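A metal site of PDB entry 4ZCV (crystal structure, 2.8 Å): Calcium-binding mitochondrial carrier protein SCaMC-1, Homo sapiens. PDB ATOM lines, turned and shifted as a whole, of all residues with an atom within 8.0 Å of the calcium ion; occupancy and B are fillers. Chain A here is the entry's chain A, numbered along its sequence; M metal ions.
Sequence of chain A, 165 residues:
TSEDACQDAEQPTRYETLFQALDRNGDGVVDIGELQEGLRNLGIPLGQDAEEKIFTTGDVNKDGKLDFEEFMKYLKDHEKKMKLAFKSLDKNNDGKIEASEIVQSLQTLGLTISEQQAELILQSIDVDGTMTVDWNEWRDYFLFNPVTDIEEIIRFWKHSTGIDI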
ATOM      1  N   PHE A  19      -6.830  19.462  23.729  1.00  0.00           N
ATOM      2  CA  PHE A  19      -8.266  19.248  23.698  1.00  0.00           C
ATOM      3  C   PHE A  19      -8.984  20.113  24.728  1.00  0.00           C
ATOM      4  O   PHE A  19      -9.966  20.776  24.406  1.00  0.00           O
ATOM      5  CB  PHE A  19      -8.587  17.763  23.938  1.00  0.00           C
ATOM      6  CG  PHE A  19     -10.037  17.429  23.803  1.00  0.00           C
ATOM      7  CD1 PHE A  19     -10.611  17.236  22.556  1.00  0.00           C
ATOM      8  CD2 PHE A  19     -10.839  17.302  24.933  1.00  0.00           C
ATOM      9  CE1 PHE A  19     -11.949  16.929  22.426  1.00  0.00           C
ATOM     10  CE2 PHE A  19     -12.183  16.997  24.811  1.00  0.00           C
ATOM     11  CZ  PHE A  19     -12.735  16.810  23.553  1.00  0.00           C
ATOM     12  N   LEU A  22      -9.079  23.612  23.668  1.00  0.00           N
ATOM     13  CA  LEU A  22     -10.081  23.877  22.628  1.00  0.00           C
ATOM     14  C   LEU A  22     -11.529  23.784  23.126  1.00  0.00           C
ATOM     15  O   LEU A  22     -12.382  24.550  22.680  1.00  0.00           O
ATOM     16  CB  LEU A  22      -9.866  22.921  21.457  1.00  0.00           C
ATOM     17  CG  LEU A  22      -8.559  23.100  20.706  1.00  0.00           C
ATOM     18  CD1 LEU A  22      -8.461  22.148  19.521  1.00  0.00           C
ATOM     19  CD2 LEU A  22      -8.391  24.545  20.253  1.00  0.00           C
ATOM     20  N   ASP A  23     -11.796  22.871  24.052  1.00  0.00           N
ATOM     21  CA  ASP A  23     -13.146  22.677  24.581  1.00  0.00           C
ATOM     22  C   ASP A  23     -13.521  23.797  25.547  1.00  0.00           C
ATOM     23  O   ASP A  23     -13.416  23.643  26.768  1.00  0.00           O
ATOM     24  CB  ASP A  23     -13.261  21.308  25.264  1.00  0.00           C
ATOM     25  CG  ASP A  23     -14.671  20.981  25.696  1.00  0.00           C
ATOM     26  OD1 ASP A  23     -15.615  21.589  25.159  1.00  0.00           O
ATOM     27  OD2 ASP A  23     -14.837  20.112  26.577  1.00  0.00           O
ATOM     28  N   ARG A  24     -13.968  24.905  24.978  1.00  0.00           N
ATOM     29  CA  ARG A  24     -14.203  26.119  25.740  1.00  0.00           C
ATOM     30  C   ARG A  24     -15.354  25.964  26.747  1.00  0.00           C
ATOM     31  O   ARG A  24     -15.258  26.441  27.878  1.00  0.00           O
ATOM     32  CB  ARG A  24     -14.461  27.277  24.771  1.00  0.00           C
ATOM     33  CG  ARG A  24     -14.064  28.623  25.318  1.00  0.00           C
ATOM     34  CD  ARG A  24     -14.558  29.783  24.473  1.00  0.00           C
ATOM     35  NE  ARG A  24     -15.984  29.688  24.210  1.00  0.00           N
ATOM     36  CZ  ARG A  24     -16.846  30.657  24.522  1.00  0.00           C
ATOM     37  NH1 ARG A  24     -16.412  31.760  25.118  1.00  0.00           N
ATOM     38  NH2 ARG A  24     -18.130  30.503  24.252  1.00  0.00           N
ATOM     39  N   ASN A  25     -16.447  25.328  26.345  1.00  0.00           N
ATOM     40  CA  ASN A  25     -17.601  25.162  27.224  1.00  0.00           C
ATOM     41  C   ASN A  25     -17.484  23.924  28.125  1.00  0.00           C
ATOM     42  O   ASN A  25     -18.368  23.645  28.927  1.00  0.00           O
ATOM     43  CB  ASN A  25     -18.908  25.093  26.421  1.00  0.00           C
ATOM     44  CG  ASN A  25     -18.941  23.926  25.469  1.00  0.00           C
ATOM     45  OD1 ASN A  25     -17.903  23.403  25.079  1.00  0.00           O
ATOM     46  ND2 ASN A  25     -20.137  23.517  25.085  1.00  0.00           N
ATOM     47  N   GLY A  26     -16.405  23.161  27.940  1.00  0.00           N
ATOM     48  CA  GLY A  26     -16.137  21.989  28.766  1.00  0.00           C
ATOM     49  C   GLY A  26     -17.189  20.892  28.701  1.00  0.00           C
ATOM     50  O   GLY A  26     -17.511  20.278  29.719  1.00  0.00           O
ATOM     51  N   ASP A  27     -17.727  20.639  27.518  1.00  0.00           N
ATOM     52  CA  ASP A  27     -18.752  19.612  27.358  1.00  0.00           C
ATOM     53  C   ASP A  27     -18.190  18.262  26.900  1.00  0.00           C
ATOM     54  O   ASP A  27     -18.937  17.315  26.683  1.00  0.00           O
ATOM     55  CB  ASP A  27     -19.819  20.092  26.368  1.00  0.00           C
ATOM     56  CG  ASP A  27     -19.257  20.368  24.986  1.00  0.00           C
ATOM     57  OD1 ASP A  27     -18.015  20.387  24.828  1.00  0.00           O
ATOM     58  OD2 ASP A  27     -20.051  20.586  24.051  1.00  0.00           O
ATOM     59  N   GLY A  28     -16.856  18.182  26.781  1.00  0.00           N
ATOM     60  CA  GLY A  28     -16.210  16.951  26.402  1.00  0.00           C
ATOM     61  C   GLY A  28     -16.038  16.760  24.899  1.00  0.00           C
ATOM     62  O   GLY A  28     -15.454  15.763  24.454  1.00  0.00           O
ATOM     63  N   VAL A  29     -16.556  17.695  24.117  1.00  0.00           N
ATOM     64  CA  VAL A  29     -16.378  17.650  22.667  1.00  0.00           C
ATOM     65  C   VAL A  29     -15.928  19.012  22.140  1.00  0.00           C
ATOM     66  O   VAL A  29     -16.102  20.027  22.809  1.00  0.00           O
ATOM     67  CB  VAL A  29     -17.663  17.238  21.909  1.00  0.00           C
ATOM     68  CG1 VAL A  29     -18.097  15.833  22.315  1.00  0.00           C
ATOM     69  CG2 VAL A  29     -18.774  18.243  22.150  1.00  0.00           C
ATOM     70  N   VAL A  30     -15.331  18.999  20.969  1.00  0.00           N
ATOM     71  CA  VAL A  30     -14.919  20.221  20.300  1.00  0.00           C
ATOM     72  C   VAL A  30     -15.784  20.451  19.066  1.00  0.00           C
ATOM     73  O   VAL A  30     -15.801  19.611  18.166  1.00  0.00           O
ATOM     74  CB  VAL A  30     -13.424  20.163  19.879  1.00  0.00           C
ATOM     75  CG1 VAL A  30     -13.092  21.309  18.934  1.00  0.00           C
ATOM     76  CG2 VAL A  30     -12.525  20.192  21.104  1.00  0.00           C
ATOM     77  N   ASP A  31     -16.517  21.555  19.044  1.00  0.00           N
ATOM     78  CA  ASP A  31     -17.293  21.910  17.867  1.00  0.00           C
ATOM     79  C   ASP A  31     -16.454  22.800  16.939  1.00  0.00           C
ATOM     80  O   ASP A  31     -15.410  23.300  17.329  1.00  0.00           O
ATOM     81  CB  ASP A  31     -18.612  22.599  18.239  1.00  0.00           C
ATOM     82  CG  ASP A  31     -18.433  23.732  19.245  1.00  0.00           C
ATOM     83  OD1 ASP A  31     -17.963  24.820  18.851  1.00  0.00           O
ATOM     84  OD2 ASP A  31     -18.771  23.530  20.428  1.00  0.00           O
ATOM     85  N   ILE A  32     -16.935  22.992  15.715  1.00  0.00           N
ATOM     86  CA  ILE A  32     -16.175  23.712  14.695  1.00  0.00           C
ATOM     87  C   ILE A  32     -15.872  25.141  15.141  1.00  0.00           C
ATOM     88  O   ILE A  32     -14.787  25.667  14.880  1.00  0.00           O
ATOM     89  CB  ILE A  32     -16.940  23.735  13.335  1.00  0.00           C
ATOM     90  CG1 ILE A  32     -16.088  24.396  12.243  1.00  0.00           C
ATOM     91  CG2 ILE A  32     -18.297  24.416  13.462  1.00  0.00           C
ATOM     92  CD1 ILE A  32     -14.764  23.706  11.978  1.00  0.00           C
ATOM     93  N   GLU A  34     -15.495  26.111  18.272  1.00  0.00           N
ATOM     94  CA  GLU A  34     -14.437  26.027  19.269  1.00  0.00           C
ATOM     95  C   GLU A  34     -13.078  25.814  18.621  1.00  0.00           C
ATOM     96  O   GLU A  34     -12.060  26.314  19.093  1.00  0.00           O
ATOM     97  CB  GLU A  34     -14.732  24.902  20.266  1.00  0.00           C
ATOM     98  CG  GLU A  34     -15.815  25.234  21.270  1.00  0.00           C
ATOM     99  CD  GLU A  34     -16.097  24.092  22.215  1.00  0.00           C
ATOM    100  OE1 GLU A  34     -15.682  22.957  21.896  1.00  0.00           O
ATOM    101  OE2 GLU A  34     -16.729  24.321  23.268  1.00  0.00           O
ATOM    102  N   LEU A  35     -13.063  25.082  17.508  1.00  0.00           N
ATOM    103  CA  LEU A  35     -11.812  24.867  16.802  1.00  0.00           C
ATOM    104  C   LEU A  35     -11.313  26.175  16.209  1.00  0.00           C
ATOM    105  O   LEU A  35     -10.132  26.510  16.315  1.00  0.00           O
ATOM    106  CB  LEU A  35     -11.990  23.807  15.718  1.00  0.00           C
ATOM    107  CG  LEU A  35     -10.709  23.432  14.963  1.00  0.00           C
ATOM    108  CD1 LEU A  35      -9.724  22.798  15.933  1.00  0.00           C
ATOM    109  CD2 LEU A  35     -11.022  22.495  13.816  1.00  0.00           C
ATOM    110  N   LYS A  65     -19.278  16.701  15.710  1.00  0.00           N
ATOM    111  CA  LYS A  65     -18.507  17.016  16.908  1.00  0.00           C
ATOM    112  C   LYS A  65     -17.213  16.224  16.920  1.00  0.00           C
ATOM    113  O   LYS A  65     -17.127  15.155  16.310  1.00  0.00           O
ATOM    114  CB  LYS A  65     -19.309  16.709  18.174  1.00  0.00           C
ATOM    115  CG  LYS A  65     -20.693  17.358  18.235  1.00  0.00           C
ATOM    116  CD  LYS A  65     -21.456  16.901  19.471  1.00  0.00           C
ATOM    117  CE  LYS A  65     -22.955  17.044  19.271  1.00  0.00           C
ATOM    118  NZ  LYS A  65     -23.740  16.469  20.398  1.00  0.00           N
ATOM    119  N   LEU A  66     -16.189  16.762  17.581  1.00  0.00           N
ATOM    120  CA  LEU A  66     -14.951  16.025  17.782  1.00  0.00           C
ATOM    121  C   LEU A  66     -14.795  15.655  19.263  1.00  0.00           C
ATOM    122  O   LEU A  66     -14.497  16.504  20.096  1.00  0.00           O
ATOM    123  CB  LEU A  66     -13.748  16.851  17.325  1.00  0.00           C
ATOM    124  CG  LEU A  66     -13.508  16.986  15.825  1.00  0.00           C
ATOM    125  CD1 LEU A  66     -12.272  17.835  15.555  1.00  0.00           C
ATOM    126  CD2 LEU A  66     -13.374  15.613  15.181  1.00  0.00           C
HETATM  127 CA    CA M   1     -17.088  22.009  23.497  1.00  0.00          CA
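The side-chain carboxylate (OD1) of Asp 23 lies close to the backbone NH (N) of Gly 26, at 3.3 Å.
The backbone NH (N) of Gly 28 sits at hydrogen-bond distance from the side-chain carboxylate (OD2) of Asp 23, at 2.8 Å.
The side-chain carboxylate (OD1) of Asp 31 sits at hydrogen-bond distance from the backbone NH (N) of Glu 34, 2.8 Å away.
The side-chain carboxylate of Glu 34 sits close to the backbone NH of Arg 24, 3.3 Å away.
OD1 of Asp 23 binds the calcium ion (2.3 Å).
The calcium ion is bound by OD1 of Asn 25 (2.3 Å).
The side-chain carboxylate (OD1) of Asp 27 binds the calcium ion (2.3 Å).
O of Val 29 is bound to the calcium ion.
The calcium ion is bound by OE1 of Glu 34, 2.3 Å away.
The calcium ion is bound by OE2 of Glu 34 (2.4 Å).
Residues that only touch the calcium ion: Asp 31.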
